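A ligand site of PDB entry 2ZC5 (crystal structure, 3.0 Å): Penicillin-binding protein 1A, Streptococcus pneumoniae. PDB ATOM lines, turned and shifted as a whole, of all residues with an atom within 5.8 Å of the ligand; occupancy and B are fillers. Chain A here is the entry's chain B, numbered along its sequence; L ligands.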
ATOM      1  N   TRP A 105      27.455  -3.010  -9.544  1.00  0.00           N
ATOM      2  CA  TRP A 105      26.681  -3.871  -8.647  1.00  0.00           C
ATOM      3  C   TRP A 105      27.296  -4.052  -7.251  1.00  0.00           C
ATOM      4  O   TRP A 105      26.796  -4.833  -6.442  1.00  0.00           O
ATOM      5  CB  TRP A 105      26.391  -5.226  -9.289  1.00  0.00           C
ATOM      6  CG  TRP A 105      25.223  -5.148 -10.199  1.00  0.00           C
ATOM      7  CD1 TRP A 105      25.202  -4.675 -11.467  1.00  0.00           C
ATOM      8  CD2 TRP A 105      23.878  -5.561  -9.901  1.00  0.00           C
ATOM      9  NE1 TRP A 105      23.938  -4.769 -11.994  1.00  0.00           N
ATOM     10  CE2 TRP A 105      23.106  -5.308 -11.059  1.00  0.00           C
ATOM     11  CE3 TRP A 105      23.257  -6.126  -8.784  1.00  0.00           C
ATOM     12  CZ2 TRP A 105      21.734  -5.588 -11.118  1.00  0.00           C
ATOM     13  CZ3 TRP A 105      21.884  -6.406  -8.844  1.00  0.00           C
ATOM     14  CH2 TRP A 105      21.152  -6.135 -10.002  1.00  0.00           C
ATOM     15  N   GLY A 106      28.388  -3.336  -7.004  1.00  0.00           N
ATOM     16  CA  GLY A 106      29.036  -3.304  -5.693  1.00  0.00           C
ATOM     17  C   GLY A 106      29.105  -4.598  -4.904  1.00  0.00           C
ATOM     18  O   GLY A 106      29.661  -5.595  -5.385  1.00  0.00           O
ATOM     19  N   SER A 107      28.522  -4.577  -3.716  1.00  0.00           N
ATOM     20  CA  SER A 107      28.659  -5.659  -2.750  1.00  0.00           C
ATOM     21  C   SER A 107      28.021  -6.983  -3.196  1.00  0.00           C
ATOM     22  O   SER A 107      28.480  -8.054  -2.784  1.00  0.00           O
ATOM     23  CB  SER A 107      28.091  -5.207  -1.398  1.00  0.00           C
ATOM     24  OG  SER A 107      28.825  -4.054  -0.885  1.00  0.00           O
ATOM     25  N   THR A 108      26.987  -6.918  -4.033  1.00  0.00           N
ATOM     26  CA  THR A 108      26.298  -8.121  -4.506  1.00  0.00           C
ATOM     27  C   THR A 108      27.238  -9.014  -5.316  1.00  0.00           C
ATOM     28  O   THR A 108      26.927 -10.180  -5.584  1.00  0.00           O
ATOM     29  CB  THR A 108      25.024  -7.799  -5.314  1.00  0.00           C
ATOM     30  OG1 THR A 108      25.376  -7.284  -6.597  1.00  0.00           O
ATOM     31  CG2 THR A 108      24.149  -6.800  -4.579  1.00  0.00           C
ATOM     32  N   LYS A 110      30.210  -9.705  -4.077  1.00  0.00           N
ATOM     33  CA  LYS A 110      30.940 -10.424  -3.016  1.00  0.00           C
ATOM     34  C   LYS A 110      30.636 -11.924  -2.969  1.00  0.00           C
ATOM     35  O   LYS A 110      31.559 -12.737  -2.997  1.00  0.00           O
ATOM     36  CB  LYS A 110      30.700  -9.808  -1.627  1.00  0.00           C
ATOM     37  CG  LYS A 110      31.330  -8.451  -1.369  1.00  0.00           C
ATOM     38  CD  LYS A 110      30.918  -7.914  -0.009  1.00  0.00           C
ATOM     39  CE  LYS A 110      31.280  -6.452   0.150  1.00  0.00           C
ATOM     40  NZ  LYS A 110      31.051  -5.940   1.521  1.00  0.00           N
ATOM     41  N   TYR A 146      38.641   0.830   2.555  1.00  0.00           N
ATOM     42  CA  TYR A 146      37.790   1.393   3.609  1.00  0.00           C
ATOM     43  C   TYR A 146      36.478   0.614   3.742  1.00  0.00           C
ATOM     44  O   TYR A 146      36.038  -0.043   2.794  1.00  0.00           O
ATOM     45  CB  TYR A 146      37.524   2.885   3.339  1.00  0.00           C
ATOM     46  CG  TYR A 146      38.771   3.748   3.360  1.00  0.00           C
ATOM     47  CD1 TYR A 146      39.392   4.134   2.174  1.00  0.00           C
ATOM     48  CD2 TYR A 146      39.330   4.173   4.565  1.00  0.00           C
ATOM     49  CE1 TYR A 146      40.544   4.923   2.184  1.00  0.00           C
ATOM     50  CE2 TYR A 146      40.483   4.960   4.589  1.00  0.00           C
ATOM     51  CZ  TYR A 146      41.087   5.334   3.395  1.00  0.00           C
ATOM     52  OH  TYR A 146      42.217   6.117   3.413  1.00  0.00           O
ATOM     53  N   ASN A 147      35.876   0.661   4.921  1.00  0.00           N
ATOM     54  CA  ASN A 147      34.500   0.203   5.072  1.00  0.00           C
ATOM     55  C   ASN A 147      33.576   1.421   5.026  1.00  0.00           C
ATOM     56  O   ASN A 147      34.025   2.542   5.226  1.00  0.00           O
ATOM     57  CB  ASN A 147      34.316  -0.571   6.374  1.00  0.00           C
ATOM     58  CG  ASN A 147      34.908  -1.967   6.311  1.00  0.00           C
ATOM     59  OD1 ASN A 147      34.835  -2.651   5.288  1.00  0.00           O
ATOM     60  ND2 ASN A 147      35.513  -2.403   7.404  1.00  0.00           N
ATOM     61  N   TRP A 148      32.296   1.184   4.743  1.00  0.00           N
ATOM     62  CA  TRP A 148      31.308   2.279   4.669  1.00  0.00           C
ATOM     63  C   TRP A 148      31.353   3.170   5.898  1.00  0.00           C
ATOM     64  O   TRP A 148      31.225   4.388   5.791  1.00  0.00           O
ATOM     65  CB  TRP A 148      29.884   1.730   4.458  1.00  0.00           C
ATOM     66  CG  TRP A 148      29.244   1.147   5.710  1.00  0.00           C
ATOM     67  CD1 TRP A 148      29.300  -0.144   6.134  1.00  0.00           C
ATOM     68  CD2 TRP A 148      28.466   1.862   6.688  1.00  0.00           C
ATOM     69  NE1 TRP A 148      28.599  -0.292   7.305  1.00  0.00           N
ATOM     70  CE2 TRP A 148      28.080   0.916   7.672  1.00  0.00           C
ATOM     71  CE3 TRP A 148      28.057   3.194   6.821  1.00  0.00           C
ATOM     72  CZ2 TRP A 148      27.303   1.278   8.783  1.00  0.00           C
ATOM     73  CZ3 TRP A 148      27.286   3.549   7.930  1.00  0.00           C
ATOM     74  CH2 TRP A 148      26.912   2.589   8.897  1.00  0.00           C
ATOM     75  N   GLN A 163      27.291 -10.606   6.273  1.00  0.00           N
ATOM     76  CA  GLN A 163      26.031 -10.042   6.756  1.00  0.00           C
ATOM     77  C   GLN A 163      26.099  -8.529   6.915  1.00  0.00           C
ATOM     78  O   GLN A 163      25.253  -7.806   6.379  1.00  0.00           O
ATOM     79  CB  GLN A 163      25.661 -10.685   8.085  1.00  0.00           C
ATOM     80  CG  GLN A 163      24.227 -10.458   8.523  1.00  0.00           C
ATOM     81  CD  GLN A 163      24.041 -10.715  10.005  1.00  0.00           C
ATOM     82  OE1 GLN A 163      23.607  -9.829  10.739  1.00  0.00           O
ATOM     83  NE2 GLN A 163      24.400 -11.914  10.463  1.00  0.00           N
ATOM     84  N   GLN A 164      27.099  -8.055   7.656  1.00  0.00           N
ATOM     85  CA  GLN A 164      27.321  -6.624   7.864  1.00  0.00           C
ATOM     86  C   GLN A 164      28.002  -6.027   6.640  1.00  0.00           C
ATOM     87  O   GLN A 164      28.093  -4.800   6.525  1.00  0.00           O
ATOM     88  CB  GLN A 164      28.165  -6.368   9.100  1.00  0.00           C
ATOM     89  CG  GLN A 164      27.551  -6.837  10.403  1.00  0.00           C
ATOM     90  CD  GLN A 164      26.186  -6.232  10.663  1.00  0.00           C
ATOM     91  OE1 GLN A 164      26.057  -5.018  10.879  1.00  0.00           O
ATOM     92  NE2 GLN A 164      25.165  -7.072  10.650  1.00  0.00           N
ATOM     93  N   SER A 165      28.484  -6.896   5.761  1.00  0.00           N
ATOM     94  CA  SER A 165      29.099  -6.519   4.473  1.00  0.00           C
ATOM     95  C   SER A 165      30.343  -5.649   4.632  1.00  0.00           C
ATOM     96  O   SER A 165      30.358  -4.462   4.294  1.00  0.00           O
ATOM     97  CB  SER A 165      28.057  -5.858   3.548  1.00  0.00           C
ATOM     98  OG  SER A 165      28.582  -5.618   2.261  1.00  0.00           O
ATOM     99  N   ASN A 167      34.217  -4.692   3.713  1.00  0.00           N
ATOM    100  CA  ASN A 167      35.019  -4.716   2.508  1.00  0.00           C
ATOM    101  C   ASN A 167      36.381  -5.354   2.694  1.00  0.00           C
ATOM    102  O   ASN A 167      36.892  -5.997   1.783  1.00  0.00           O
ATOM    103  CB  ASN A 167      35.135  -3.324   1.892  1.00  0.00           C
ATOM    104  CG  ASN A 167      33.788  -2.779   1.404  1.00  0.00           C
ATOM    105  OD1 ASN A 167      32.897  -3.536   1.006  1.00  0.00           O
ATOM    106  ND2 ASN A 167      33.636  -1.471   1.456  1.00  0.00           N
ATOM    107  N   ILE A 202      34.710  -6.022  -4.659  1.00  0.00           N
ATOM    108  CA  ILE A 202      33.612  -5.210  -4.122  1.00  0.00           C
ATOM    109  C   ILE A 202      32.914  -4.346  -5.193  1.00  0.00           C
ATOM    110  O   ILE A 202      32.243  -3.367  -4.872  1.00  0.00           O
ATOM    111  CB  ILE A 202      34.062  -4.315  -2.917  1.00  0.00           C
ATOM    112  CG1 ILE A 202      35.193  -3.362  -3.325  1.00  0.00           C
ATOM    113  CG2 ILE A 202      34.428  -5.176  -1.705  1.00  0.00           C
ATOM    114  CD1 ILE A 202      35.321  -2.111  -2.442  1.00  0.00           C
ATOM    115  N   GLY A 279      20.826  -8.482   9.327  1.00  0.00           N
ATOM    116  CA  GLY A 279      21.651  -7.419   8.779  1.00  0.00           C
ATOM    117  C   GLY A 279      20.922  -6.426   7.895  1.00  0.00           C
ATOM    118  O   GLY A 279      19.950  -5.789   8.324  1.00  0.00           O
ATOM    119  N   THR A 280      21.402  -6.337   6.660  1.00  0.00           N
ATOM    120  CA  THR A 280      21.100  -5.243   5.744  1.00  0.00           C
ATOM    121  C   THR A 280      19.692  -5.288   5.121  1.00  0.00           C
ATOM    122  O   THR A 280      18.864  -4.389   5.349  1.00  0.00           O
ATOM    123  CB  THR A 280      22.207  -5.123   4.645  1.00  0.00           C
ATOM    124  OG1 THR A 280      22.324  -6.373   3.944  1.00  0.00           O
ATOM    125  CG2 THR A 280      23.559  -4.826   5.282  1.00  0.00           C
ATOM    126  N   LYS A 294      21.739 -10.749  -0.992  1.00  0.00           N
ATOM    127  CA  LYS A 294      22.778  -9.801  -0.626  1.00  0.00           C
ATOM    128  C   LYS A 294      22.392  -8.407  -1.124  1.00  0.00           C
ATOM    129  O   LYS A 294      21.875  -8.262  -2.225  1.00  0.00           O
ATOM    130  CB  LYS A 294      24.133 -10.228  -1.211  1.00  0.00           C
ATOM    131  CG  LYS A 294      25.320  -9.268  -0.962  1.00  0.00           C
ATOM    132  CD  LYS A 294      25.991  -9.449   0.401  1.00  0.00           C
ATOM    133  CE  LYS A 294      25.597  -8.367   1.398  1.00  0.00           C
ATOM    134  NZ  LYS A 294      26.299  -7.094   1.107  1.00  0.00           N
ATOM    135  N   THR A 295      22.643  -7.412  -0.283  1.00  0.00           N
ATOM    136  CA  THR A 295      22.382  -6.013  -0.639  1.00  0.00           C
ATOM    137  C   THR A 295      23.618  -5.386  -1.262  1.00  0.00           C
ATOM    138  O   THR A 295      24.725  -5.914  -1.147  1.00  0.00           O
ATOM    139  CB  THR A 295      22.001  -5.188   0.577  1.00  0.00           C
ATOM    140  OG1 THR A 295      22.934  -5.444   1.629  1.00  0.00           O
ATOM    141  CG2 THR A 295      20.599  -5.539   1.047  1.00  0.00           C
ATOM    142  N   GLY A 296      23.423  -4.248  -1.914  1.00  0.00           N
ATOM    143  CA  GLY A 296      24.506  -3.529  -2.562  1.00  0.00           C
ATOM    144  C   GLY A 296      24.264  -2.047  -2.570  1.00  0.00           C
ATOM    145  O   GLY A 296      23.170  -1.582  -2.889  1.00  0.00           O
ATOM    146  N   THR A 297      25.304  -1.295  -2.198  1.00  0.00           N
ATOM    147  CA  THR A 297      25.265   0.159  -2.226  1.00  0.00           C
ATOM    148  C   THR A 297      26.595   0.651  -2.770  1.00  0.00           C
ATOM    149  O   THR A 297      27.539   0.840  -2.003  1.00  0.00           O
ATOM    150  CB  THR A 297      25.039   0.756  -0.813  1.00  0.00           C
ATOM    151  OG1 THR A 297      24.118  -0.059  -0.077  1.00  0.00           O
ATOM    152  CG2 THR A 297      24.499   2.173  -0.901  1.00  0.00           C
ATOM    153  N   SER A 298      26.670   0.845  -4.073  1.00  0.00           N
ATOM    154  CA  SER A 298      27.882   1.355  -4.719  1.00  0.00           C
ATOM    155  C   SER A 298      28.220   2.784  -4.249  1.00  0.00           C
ATOM    156  O   SER A 298      27.415   3.422  -3.560  1.00  0.00           O
ATOM    157  CB  SER A 298      27.767   1.287  -6.241  1.00  0.00           C
ATOM    158  OG  SER A 298      26.900   2.286  -6.748  1.00  0.00           O
ATOM    159  N   ASN A 299      29.406   3.278  -4.616  1.00  0.00           N
ATOM    160  CA  ASN A 299      29.800   4.641  -4.232  1.00  0.00           C
ATOM    161  C   ASN A 299      30.332   5.469  -5.395  1.00  0.00           C
ATOM    162  O   ASN A 299      30.503   4.971  -6.502  1.00  0.00           O
ATOM    163  CB  ASN A 299      30.780   4.614  -3.048  1.00  0.00           C
ATOM    164  CG  ASN A 299      31.991   3.746  -3.323  1.00  0.00           C
ATOM    165  OD1 ASN A 299      32.767   3.991  -4.241  1.00  0.00           O
ATOM    166  ND2 ASN A 299      32.168   2.713  -2.496  1.00  0.00           N
ATOM    167  N   PHE A 314      24.512  10.093   3.770  1.00  0.00           N
ATOM    168  CA  PHE A 314      24.809   8.817   3.137  1.00  0.00           C
ATOM    169  C   PHE A 314      24.094   8.779   1.788  1.00  0.00           C
ATOM    170  O   PHE A 314      22.869   8.747   1.726  1.00  0.00           O
ATOM    171  CB  PHE A 314      24.354   7.676   4.046  1.00  0.00           C
ATOM    172  CG  PHE A 314      24.885   6.331   3.637  1.00  0.00           C
ATOM    173  CD1 PHE A 314      26.101   5.872   4.142  1.00  0.00           C
ATOM    174  CD2 PHE A 314      24.160   5.504   2.785  1.00  0.00           C
ATOM    175  CE1 PHE A 314      26.594   4.618   3.778  1.00  0.00           C
ATOM    176  CE2 PHE A 314      24.641   4.243   2.407  1.00  0.00           C
ATOM    177  CZ  PHE A 314      25.861   3.801   2.914  1.00  0.00           C
ATOM    178  N   GLU A 319      21.677   1.404  -5.822  1.00  0.00           N
ATOM    179  CA  GLU A 319      21.319   0.507  -4.719  1.00  0.00           C
ATOM    180  C   GLU A 319      20.814  -0.795  -5.315  1.00  0.00           C
ATOM    181  O   GLU A 319      20.025  -0.783  -6.264  1.00  0.00           O
ATOM    182  CB  GLU A 319      20.262   1.144  -3.817  1.00  0.00           C
ATOM    183  CG  GLU A 319      19.630   0.211  -2.784  1.00  0.00           C
ATOM    184  CD  GLU A 319      20.588  -0.219  -1.675  1.00  0.00           C
ATOM    185  OE1 GLU A 319      21.374   0.634  -1.204  1.00  0.00           O
ATOM    186  OE2 GLU A 319      20.532  -1.403  -1.262  1.00  0.00           O
ATOM    187  N   LEU A 320      21.263  -1.918  -4.759  1.00  0.00           N
ATOM    188  CA  LEU A 320      21.047  -3.232  -5.372  1.00  0.00           C
ATOM    189  C   LEU A 320      20.564  -4.283  -4.383  1.00  0.00           C
ATOM    190  O   LEU A 320      20.913  -4.254  -3.208  1.00  0.00           O
ATOM    191  CB  LEU A 320      22.340  -3.737  -6.007  1.00  0.00           C
ATOM    192  CG  LEU A 320      23.116  -2.659  -6.756  1.00  0.00           C
ATOM    193  CD1 LEU A 320      24.542  -2.607  -6.276  1.00  0.00           C
ATOM    194  CD2 LEU A 320      23.003  -2.832  -8.258  1.00  0.00           C
HETATM  195  C1  LIG L   1      28.160  -0.702   2.027  1.00  0.00           C
HETATM  196  C2  LIG L   1      26.413  -2.266   1.780  1.00  0.00           C
HETATM  197  C3  LIG L   1      28.683  -1.970   1.228  1.00  0.00           C
HETATM  198  C4  LIG L   1      29.074  -1.768  -0.263  1.00  0.00           C
HETATM  199  C5  LIG L   1      28.444  -2.781  -1.164  1.00  0.00           C
HETATM  200  C6  LIG L   1      30.596  -1.775  -0.488  1.00  0.00           C
HETATM  201  C7  LIG L   1      25.096  -3.090   1.619  1.00  0.00           C
HETATM  202  C8  LIG L   1      25.327  -0.739   4.612  1.00  0.00           C
HETATM  203  C9  LIG L   1      25.348   0.337   5.734  1.00  0.00           C
HETATM  204  C10 LIG L   1      24.865  -0.691   8.140  1.00  0.00           C
HETATM  205  C11 LIG L   1      23.626  -2.240   7.347  1.00  0.00           C
HETATM  206  C12 LIG L   1      31.012  -1.548  -1.942  1.00  0.00           C
HETATM  207  O1  LIG L   1      27.682  -2.508  -2.076  1.00  0.00           O
HETATM  208  O2  LIG L   1      31.136  -0.712   0.327  1.00  0.00           O
HETATM  209  C13 LIG L   1      28.314   0.658   1.339  1.00  0.00           C
HETATM  210  N1  LIG L   1      27.575  -2.905   1.401  1.00  0.00           N
HETATM  211  O3  LIG L   1      25.253  -4.315   1.802  1.00  0.00           O
HETATM  212  O4  LIG L   1      24.058  -2.446   1.337  1.00  0.00           O
HETATM  213  C14 LIG L   1      26.670  -1.041   2.233  1.00  0.00           C
HETATM  214  S1  LIG L   1      25.528   0.054   2.981  1.00  0.00           S
HETATM  215  C15 LIG L   1      23.951  -1.417   4.822  1.00  0.00           C
HETATM  216  N2  LIG L   1      24.040  -1.521   6.320  1.00  0.00           N
HETATM  217  N3  LIG L   1      24.831  -0.530   6.833  1.00  0.00           N
HETATM  218  N4  LIG L   1      24.130  -1.743   8.496  1.00  0.00           N
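C of Gly 106 touches O1 of the ligand, 3.8 Å away.
Trp 148 touches the ligand (CZ2 to C10, 3.2 Å).
Ile 202 touches the ligand.
CG2 of Thr 280 touches C11 of the ligand, 3.3 Å away.
Gly 296 touches the ligand (CA to O1, 3.4 Å).
Phe 314 touches the ligand (CZ to S1, 3.8 Å).
The nearest printed residue that does not touch the ligand is Ser 298 (4.03 Å).
The backbone NH (N) of Thr 297 lies within hydrogen-bond range of an oxygen (O1) of the ligand, 2.7 Å away.
The backbone NH (N) of Ser 107 is in hydrogen-bond range of an oxygen (O1) of the ligand (2.8 Å).
An oxygen (O4) of the ligand is in hydrogen-bond range of the side-chain hydroxyl (OG1) of Thr 297.
The side-chain amino group (NZ) of Lys 294 is in salt-bridge range of an oxygen (O3) of the ligand, 3.0 Å away.
O3 of the ligand is in hydrogen-bond range of OG1 of Thr 295, at 2.6 Å.
OG of Ser 107 is covalently linked to C5 of the ligand, at 1.4 Å.
The side-chain hydroxyl (OG) of Ser 165 sits at hydrogen-bond distance from a nitrogen (N1) of the ligand (3.0 Å).
The side-chain amide nitrogen (ND2) of Asn 167 sits at hydrogen-bond distance from an oxygen (O2) of the ligand (2.8 Å).
The backbone NH (N) of Leu 320 sits at hydrogen-bond distance from the backbone carbonyl oxygen (O) of Gly 296, at 2.7 Å.
N of Asn 167 sits at hydrogen-bond distance from OD1 of Asn 147.
The side-chain hydroxyl (OG1) of Thr 297 lies within hydrogen-bond range of the side-chain carboxylate (OE1) of Glu 319, at 3.0 Å.
The side-chain amino group (NZ) of Lys 110 is in hydrogen-bond range of the side-chain hydroxyl (OG) of Ser 165 (2.6 Å).
The side-chain hydroxyl (OG) of Ser 165 lies within hydrogen-bond range of the side-chain amino group (NZ) of Lys 294, 3.0 Å away.
The side-chain amino group (NZ) of Lys 110 lies within hydrogen-bond range of the side-chain amide oxygen (OD1) of Asn 167 (3.1 Å).
OG1 of Thr 295 is in hydrogen-bond range of OG1 of Thr 280 (2.6 Å).
The side-chain amide nitrogen (ND2) of Asn 167 lies within hydrogen-bond range of the backbone carbonyl oxygen (O) of Tyr 146.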
